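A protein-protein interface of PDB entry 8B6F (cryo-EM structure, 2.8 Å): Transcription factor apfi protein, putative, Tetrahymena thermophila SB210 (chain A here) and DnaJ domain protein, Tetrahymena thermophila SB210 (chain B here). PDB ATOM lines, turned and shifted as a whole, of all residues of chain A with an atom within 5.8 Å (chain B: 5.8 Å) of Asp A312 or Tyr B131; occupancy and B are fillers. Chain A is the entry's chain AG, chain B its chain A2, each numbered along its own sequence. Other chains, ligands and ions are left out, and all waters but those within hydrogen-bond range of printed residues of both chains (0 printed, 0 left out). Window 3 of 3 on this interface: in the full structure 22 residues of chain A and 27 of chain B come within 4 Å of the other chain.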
ATOM      1  N   ASN A 286     -17.096 -16.014 -12.710  1.00  0.00           N
ATOM      2  CA  ASN A 286     -15.821 -15.669 -12.103  1.00  0.00           C
ATOM      3  C   ASN A 286     -15.226 -14.464 -12.813  1.00  0.00           C
ATOM      4  O   ASN A 286     -15.381 -14.297 -14.025  1.00  0.00           O
ATOM      5  CB  ASN A 286     -14.844 -16.847 -12.163  1.00  0.00           C
ATOM      6  CG  ASN A 286     -13.627 -16.637 -11.296  1.00  0.00           C
ATOM      7  OD1 ASN A 286     -13.636 -15.814 -10.382  1.00  0.00           O
ATOM      8  ND2 ASN A 286     -12.569 -17.386 -11.572  1.00  0.00           N
ATOM      9  N   ASP A 288     -11.797 -13.572 -12.052  1.00  0.00           N
ATOM     10  CA  ASP A 288     -10.359 -13.633 -11.867  1.00  0.00           C
ATOM     11  C   ASP A 288      -9.647 -13.308 -13.179  1.00  0.00           C
ATOM     12  O   ASP A 288     -10.137 -13.646 -14.260  1.00  0.00           O
ATOM     13  CB  ASP A 288      -9.936 -15.015 -11.381  1.00  0.00           C
ATOM     14  CG  ASP A 288     -10.416 -15.309  -9.976  1.00  0.00           C
ATOM     15  OD1 ASP A 288     -11.070 -14.432  -9.376  1.00  0.00           O
ATOM     16  OD2 ASP A 288     -10.138 -16.416  -9.470  1.00  0.00           O
ATOM     17  N   GLN A 306      -2.570 -20.241 -10.360  1.00  0.00           N
ATOM     18  CA  GLN A 306      -3.345 -19.815  -9.204  1.00  0.00           C
ATOM     19  C   GLN A 306      -3.546 -20.986  -8.250  1.00  0.00           C
ATOM     20  O   GLN A 306      -3.808 -22.115  -8.670  1.00  0.00           O
ATOM     21  CB  GLN A 306      -4.693 -19.251  -9.652  1.00  0.00           C
ATOM     22  CG  GLN A 306      -5.588 -18.786  -8.513  1.00  0.00           C
ATOM     23  CD  GLN A 306      -6.901 -18.212  -9.006  1.00  0.00           C
ATOM     24  OE1 GLN A 306      -7.971 -18.575  -8.521  1.00  0.00           O
ATOM     25  NE2 GLN A 306      -6.825 -17.301  -9.970  1.00  0.00           N
ATOM     26  N   GLN A 307      -3.418 -20.711  -6.955  1.00  0.00           N
ATOM     27  CA  GLN A 307      -3.451 -21.755  -5.933  1.00  0.00           C
ATOM     28  C   GLN A 307      -4.900 -22.104  -5.624  1.00  0.00           C
ATOM     29  O   GLN A 307      -5.580 -21.393  -4.883  1.00  0.00           O
ATOM     30  CB  GLN A 307      -2.716 -21.297  -4.679  1.00  0.00           C
ATOM     31  CG  GLN A 307      -1.253 -20.975  -4.916  1.00  0.00           C
ATOM     32  CD  GLN A 307      -0.469 -22.172  -5.412  1.00  0.00           C
ATOM     33  OE1 GLN A 307      -0.782 -23.314  -5.076  1.00  0.00           O
ATOM     34  NE2 GLN A 307       0.550 -21.919  -6.223  1.00  0.00           N
ATOM     35  N   TYR A 308      -5.370 -23.216  -6.189  1.00  0.00           N
ATOM     36  CA  TYR A 308      -6.731 -23.671  -5.941  1.00  0.00           C
ATOM     37  C   TYR A 308      -6.873 -24.330  -4.576  1.00  0.00           C
ATOM     38  O   TYR A 308      -7.972 -24.345  -4.011  1.00  0.00           O
ATOM     39  CB  TYR A 308      -7.161 -24.646  -7.034  1.00  0.00           C
ATOM     40  CG  TYR A 308      -6.884 -24.148  -8.432  1.00  0.00           C
ATOM     41  CD1 TYR A 308      -7.119 -22.823  -8.776  1.00  0.00           C
ATOM     42  CD2 TYR A 308      -6.370 -24.996  -9.400  1.00  0.00           C
ATOM     43  CE1 TYR A 308      -6.861 -22.363 -10.050  1.00  0.00           C
ATOM     44  CE2 TYR A 308      -6.109 -24.546 -10.676  1.00  0.00           C
ATOM     45  CZ  TYR A 308      -6.358 -23.229 -10.996  1.00  0.00           C
ATOM     46  OH  TYR A 308      -6.098 -22.775 -12.266  1.00  0.00           O
ATOM     47  N   LYS A 309      -5.783 -24.874  -4.033  1.00  0.00           N
ATOM     48  CA  LYS A 309      -5.845 -25.481  -2.709  1.00  0.00           C
ATOM     49  C   LYS A 309      -6.188 -24.445  -1.648  1.00  0.00           C
ATOM     50  O   LYS A 309      -6.913 -24.741  -0.692  1.00  0.00           O
ATOM     51  CB  LYS A 309      -4.523 -26.173  -2.385  1.00  0.00           C
ATOM     52  CG  LYS A 309      -4.219 -27.349  -3.298  1.00  0.00           C
ATOM     53  CD  LYS A 309      -2.968 -28.091  -2.862  1.00  0.00           C
ATOM     54  CE  LYS A 309      -2.653 -29.244  -3.802  1.00  0.00           C
ATOM     55  NZ  LYS A 309      -3.766 -30.232  -3.882  1.00  0.00           N
ATOM     56  N   ARG A 310      -5.677 -23.223  -1.798  1.00  0.00           N
ATOM     57  CA  ARG A 310      -6.031 -22.164  -0.860  1.00  0.00           C
ATOM     58  C   ARG A 310      -7.521 -21.857  -0.923  1.00  0.00           C
ATOM     59  O   ARG A 310      -8.160 -21.641   0.113  1.00  0.00           O
ATOM     60  CB  ARG A 310      -5.207 -20.909  -1.152  1.00  0.00           C
ATOM     61  CG  ARG A 310      -3.715 -21.078  -0.896  1.00  0.00           C
ATOM     62  CD  ARG A 310      -3.430 -21.470   0.547  1.00  0.00           C
ATOM     63  NE  ARG A 310      -2.003 -21.480   0.846  1.00  0.00           N
ATOM     64  CZ  ARG A 310      -1.313 -20.430   1.270  1.00  0.00           C
ATOM     65  NH1 ARG A 310      -1.883 -19.248   1.441  1.00  0.00           N
ATOM     66  NH2 ARG A 310      -0.016 -20.569   1.528  1.00  0.00           N
ATOM     67  N   TYR A 311      -8.094 -21.827  -2.127  1.00  0.00           N
ATOM     68  CA  TYR A 311      -9.531 -21.608  -2.244  1.00  0.00           C
ATOM     69  C   TYR A 311     -10.312 -22.731  -1.577  1.00  0.00           C
ATOM     70  O   TYR A 311     -11.303 -22.480  -0.882  1.00  0.00           O
ATOM     71  CB  TYR A 311      -9.927 -21.484  -3.715  1.00  0.00           C
ATOM     72  CG  TYR A 311      -9.531 -20.169  -4.340  1.00  0.00           C
ATOM     73  CD1 TYR A 311      -8.275 -19.994  -4.899  1.00  0.00           C
ATOM     74  CD2 TYR A 311     -10.419 -19.102  -4.374  1.00  0.00           C
ATOM     75  CE1 TYR A 311      -7.910 -18.794  -5.473  1.00  0.00           C
ATOM     76  CE2 TYR A 311     -10.065 -17.898  -4.945  1.00  0.00           C
ATOM     77  CZ  TYR A 311      -8.808 -17.750  -5.493  1.00  0.00           C
ATOM     78  OH  TYR A 311      -8.449 -16.552  -6.063  1.00  0.00           O
ATOM     79  N   ASP A 312      -9.890 -23.981  -1.781  1.00  0.00           N
ATOM     80  CA  ASP A 312     -10.580 -25.100  -1.148  1.00  0.00           C
ATOM     81  C   ASP A 312     -10.496 -25.010   0.370  1.00  0.00           C
ATOM     82  O   ASP A 312     -11.486 -25.255   1.069  1.00  0.00           O
ATOM     83  CB  ASP A 312      -9.994 -26.423  -1.639  1.00  0.00           C
ATOM     84  CG  ASP A 312     -10.236 -26.654  -3.117  1.00  0.00           C
ATOM     85  OD1 ASP A 312     -11.260 -26.165  -3.636  1.00  0.00           O
ATOM     86  OD2 ASP A 312      -9.402 -27.323  -3.760  1.00  0.00           O
ATOM     87  N   GLU A 313      -9.317 -24.678   0.899  1.00  0.00           N
ATOM     88  CA  GLU A 313      -9.160 -24.561   2.344  1.00  0.00           C
ATOM     89  C   GLU A 313     -10.003 -23.422   2.902  1.00  0.00           C
ATOM     90  O   GLU A 313     -10.618 -23.557   3.966  1.00  0.00           O
ATOM     91  CB  GLU A 313      -7.687 -24.355   2.692  1.00  0.00           C
ATOM     92  CG  GLU A 313      -6.810 -25.545   2.346  1.00  0.00           C
ATOM     93  CD  GLU A 313      -5.334 -25.227   2.447  1.00  0.00           C
ATOM     94  OE1 GLU A 313      -4.994 -24.122   2.917  1.00  0.00           O
ATOM     95  OE2 GLU A 313      -4.512 -26.081   2.054  1.00  0.00           O
ATOM     96  N   ALA A 314     -10.041 -22.289   2.199  1.00  0.00           N
ATOM     97  CA  ALA A 314     -10.864 -21.172   2.649  1.00  0.00           C
ATOM     98  C   ALA A 314     -12.340 -21.540   2.642  1.00  0.00           C
ATOM     99  O   ALA A 314     -13.078 -21.196   3.571  1.00  0.00           O
ATOM    100  CB  ALA A 314     -10.609 -19.949   1.771  1.00  0.00           C
ATOM    101  N   LYS A 315     -12.790 -22.246   1.602  1.00  0.00           N
ATOM    102  CA  LYS A 315     -14.179 -22.686   1.562  1.00  0.00           C
ATOM    103  C   LYS A 315     -14.489 -23.608   2.734  1.00  0.00           C
ATOM    104  O   LYS A 315     -15.539 -23.478   3.375  1.00  0.00           O
ATOM    105  CB  LYS A 315     -14.471 -23.385   0.235  1.00  0.00           C
ATOM    106  CG  LYS A 315     -15.871 -23.973   0.144  1.00  0.00           C
ATOM    107  CD  LYS A 315     -16.169 -24.491  -1.254  1.00  0.00           C
ATOM    108  CE  LYS A 315     -17.546 -25.130  -1.318  1.00  0.00           C
ATOM    109  NZ  LYS A 315     -17.889 -25.583  -2.693  1.00  0.00           N
ATOM    110  N   LYS A 316     -13.588 -24.544   3.029  1.00  0.00           N
ATOM    111  CA  LYS A 316     -13.793 -25.430   4.169  1.00  0.00           C
ATOM    112  C   LYS A 316     -13.873 -24.638   5.467  1.00  0.00           C
ATOM    113  O   LYS A 316     -14.746 -24.889   6.304  1.00  0.00           O
ATOM    114  CB  LYS A 316     -12.666 -26.460   4.237  1.00  0.00           C
ATOM    115  CG  LYS A 316     -12.840 -27.504   5.333  1.00  0.00           C
ATOM    116  CD  LYS A 316     -11.595 -28.368   5.493  1.00  0.00           C
ATOM    117  CE  LYS A 316     -11.306 -29.200   4.250  1.00  0.00           C
ATOM    118  NZ  LYS A 316     -12.423 -30.122   3.910  1.00  0.00           N
ATOM    119  N   TYR A 317     -12.971 -23.673   5.651  1.00  0.00           N
ATOM    120  CA  TYR A 317     -12.963 -22.892   6.883  1.00  0.00           C
ATOM    121  C   TYR A 317     -14.246 -22.090   7.048  1.00  0.00           C
ATOM    122  O   TYR A 317     -14.810 -22.026   8.146  1.00  0.00           O
ATOM    123  CB  TYR A 317     -11.751 -21.960   6.904  1.00  0.00           C
ATOM    124  CG  TYR A 317     -11.781 -20.968   8.041  1.00  0.00           C
ATOM    125  CD1 TYR A 317     -11.325 -21.316   9.304  1.00  0.00           C
ATOM    126  CD2 TYR A 317     -12.270 -19.683   7.851  1.00  0.00           C
ATOM    127  CE1 TYR A 317     -11.354 -20.411  10.347  1.00  0.00           C
ATOM    128  CE2 TYR A 317     -12.302 -18.771   8.886  1.00  0.00           C
ATOM    129  CZ  TYR A 317     -11.842 -19.141  10.131  1.00  0.00           C
ATOM    130  OH  TYR A 317     -11.875 -18.237  11.167  1.00  0.00           O
ATOM    131  N   GLY B 129     -16.048 -31.341  -8.373  1.00  0.00           N
ATOM    132  CA  GLY B 129     -16.421 -30.466  -7.281  1.00  0.00           C
ATOM    133  C   GLY B 129     -15.283 -29.664  -6.695  1.00  0.00           C
ATOM    134  O   GLY B 129     -15.388 -29.210  -5.552  1.00  0.00           O
ATOM    135  N   THR B 130     -14.201 -29.474  -7.440  1.00  0.00           N
ATOM    136  CA  THR B 130     -13.032 -28.743  -6.977  1.00  0.00           C
ATOM    137  C   THR B 130     -12.890 -27.435  -7.742  1.00  0.00           C
ATOM    138  O   THR B 130     -13.236 -27.344  -8.921  1.00  0.00           O
ATOM    139  CB  THR B 130     -11.754 -29.570  -7.137  1.00  0.00           C
ATOM    140  OG1 THR B 130     -11.694 -30.120  -8.459  1.00  0.00           O
ATOM    141  CG2 THR B 130     -11.714 -30.692  -6.115  1.00  0.00           C
ATOM    142  N   TYR B 131     -12.375 -26.419  -7.050  1.00  0.00           N
ATOM    143  CA  TYR B 131     -12.123 -25.138  -7.696  1.00  0.00           C
ATOM    144  C   TYR B 131     -11.193 -25.296  -8.890  1.00  0.00           C
ATOM    145  O   TYR B 131     -11.279 -24.523  -9.850  1.00  0.00           O
ATOM    146  CB  TYR B 131     -11.532 -24.152  -6.689  1.00  0.00           C
ATOM    147  CG  TYR B 131     -11.468 -22.729  -7.192  1.00  0.00           C
ATOM    148  CD1 TYR B 131     -10.369 -22.272  -7.905  1.00  0.00           C
ATOM    149  CD2 TYR B 131     -12.506 -21.842  -6.950  1.00  0.00           C
ATOM    150  CE1 TYR B 131     -10.307 -20.971  -8.365  1.00  0.00           C
ATOM    151  CE2 TYR B 131     -12.454 -20.540  -7.405  1.00  0.00           C
ATOM    152  CZ  TYR B 131     -11.352 -20.111  -8.111  1.00  0.00           C
ATOM    153  OH  TYR B 131     -11.297 -18.814  -8.565  1.00  0.00           O
ATOM    154  N   ALA B 132     -10.299 -26.283  -8.849  1.00  0.00           N
ATOM    155  CA  ALA B 132      -9.416 -26.529  -9.982  1.00  0.00           C
ATOM    156  C   ALA B 132     -10.215 -26.916 -11.219  1.00  0.00           C
ATOM    157  O   ALA B 132      -9.983 -26.388 -12.312  1.00  0.00           O
ATOM    158  CB  ALA B 132      -8.404 -27.620  -9.632  1.00  0.00           C
ATOM    159  N   ALA B 133     -11.160 -27.846 -11.068  1.00  0.00           N
ATOM    160  CA  ALA B 133     -11.983 -28.238 -12.206  1.00  0.00           C
ATOM    161  C   ALA B 133     -12.844 -27.076 -12.686  1.00  0.00           C
ATOM    162  O   ALA B 133     -12.992 -26.863 -13.895  1.00  0.00           O
ATOM    163  CB  ALA B 133     -12.858 -29.433 -11.836  1.00  0.00           C
ATOM    164  N   GLU B 134     -13.421 -26.316 -11.756  1.00  0.00           N
ATOM    165  CA  GLU B 134     -14.247 -25.177 -12.140  1.00  0.00           C
ATOM    166  C   GLU B 134     -13.435 -24.160 -12.931  1.00  0.00           C
ATOM    167  O   GLU B 134     -13.882 -23.661 -13.969  1.00  0.00           O
ATOM    168  CB  GLU B 134     -14.857 -24.527 -10.898  1.00  0.00           C
ATOM    169  CG  GLU B 134     -15.866 -23.432 -11.214  1.00  0.00           C
ATOM    170  CD  GLU B 134     -16.443 -22.795  -9.966  1.00  0.00           C
ATOM    171  OE1 GLU B 134     -15.917 -23.061  -8.865  1.00  0.00           O
ATOM    172  OE2 GLU B 134     -17.423 -22.028 -10.084  1.00  0.00           O
ATOM    173  N   LYS B 135     -12.230 -23.848 -12.455  1.00  0.00           N
ATOM    174  CA  LYS B 135     -11.387 -22.878 -13.145  1.00  0.00           C
ATOM    175  C   LYS B 135     -10.942 -23.407 -14.503  1.00  0.00           C
ATOM    176  O   LYS B 135     -10.829 -22.641 -15.465  1.00  0.00           O
ATOM    177  CB  LYS B 135     -10.179 -22.527 -12.279  1.00  0.00           C
ATOM    178  CG  LYS B 135      -9.490 -21.224 -12.662  1.00  0.00           C
ATOM    179  CD  LYS B 135     -10.344 -20.015 -12.312  1.00  0.00           C
ATOM    180  CE  LYS B 135      -9.584 -18.717 -12.528  1.00  0.00           C
ATOM    181  NZ  LYS B 135      -9.169 -18.535 -13.945  1.00  0.00           N
ATOM    182  N   GLN B 136     -10.690 -24.712 -14.602  1.00  0.00           N
ATOM    183  CA  GLN B 136     -10.333 -25.292 -15.892  1.00  0.00           C
ATOM    184  C   GLN B 136     -11.463 -25.122 -16.901  1.00  0.00           C
ATOM    185  O   GLN B 136     -11.219 -24.761 -18.058  1.00  0.00           O
ATOM    186  CB  GLN B 136      -9.975 -26.767 -15.718  1.00  0.00           C
ATOM    187  CG  GLN B 136      -9.431 -27.422 -16.978  1.00  0.00           C
ATOM    188  CD  GLN B 136      -8.790 -28.764 -16.701  1.00  0.00           C
ATOM    189  OE1 GLN B 136      -8.797 -29.246 -15.570  1.00  0.00           O
ATOM    190  NE2 GLN B 136      -8.226 -29.375 -17.735  1.00  0.00           N
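The side-chain amide oxygen (OD1) of Asn A286 sits close to the side-chain carboxylate (OD1) of Asp A288.
The side-chain carboxylate (OD2) of Asp A288 sits close to the side-chain amide oxygen (OE1) of Gln A306 (3.2 Å).
The side-chain hydroxyl (OH) of Tyr A311 lies close to the side-chain amide oxygen (OE1) of Gln A306 (3.2 Å).
Hydrophobic or aromatic side chains of chain A that line the printed part of chain B: Tyr A308 and Tyr A311.
Hydrophobic or aromatic side chains of chain B within 4 Å of the printed part of chain A: Tyr B131 and Ala B132.
Among the printed residues, no Asp or Glu carboxylate lies within 4 Å of a Lys or Arg side-chain nitrogen of the other chain.
Of chain B, only Tyr B131 (3.6 Å) comes within 4 Å of Asp A312.
Tyr B131 touches just these residues of chain A: Asn A286 (3.6 Å), Asp A288 (2.8 Å), Gln A306 (3.3 Å), Tyr A308 (3.4 Å), Tyr A311 (3.9 Å) and Asp A312 (3.6 Å).
Of the printed residues of chain A, Ala B132 touches Tyr A308 (3.3 Å).
Printed residues of chain B within 4 Å of Gln A306: Tyr B131.
Of the printed residues of chain B, Tyr A311 touches Tyr B131.
Of the printed residues of chain B, Tyr A308 touches Tyr B131 (3.4 Å), Ala B132 (3.3 Å) and Lys B135 (3.8 Å).
Of the printed residues of chain B, Asp A288 touches Tyr B131 (2.8 Å) and Lys B135 (3.9 Å).
Tyr A317 touches none of the printed residues of chain B.
Among the printed residues, merely in contact across the chains: Asn A286 with Tyr B131 (3.6 Å), Asn A286 with Lys B135 (3.4 Å), Asp A288 with Lys B135 (3.9 Å), Tyr A308 with Tyr B131 (3.4 Å), Tyr A308 with Ala B132 (3.3 Å), Tyr A308 with Lys B135 (3.8 Å), Tyr A311 with Tyr B131 (3.9 Å) and Asp A312 with Tyr B131 (3.6 Å).
OH of Tyr B131 sits at hydrogen-bond distance from OD2 of Asp A288.
OH of Tyr B131 is in hydrogen-bond range of OE1 of Gln A306 (3.3 Å).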
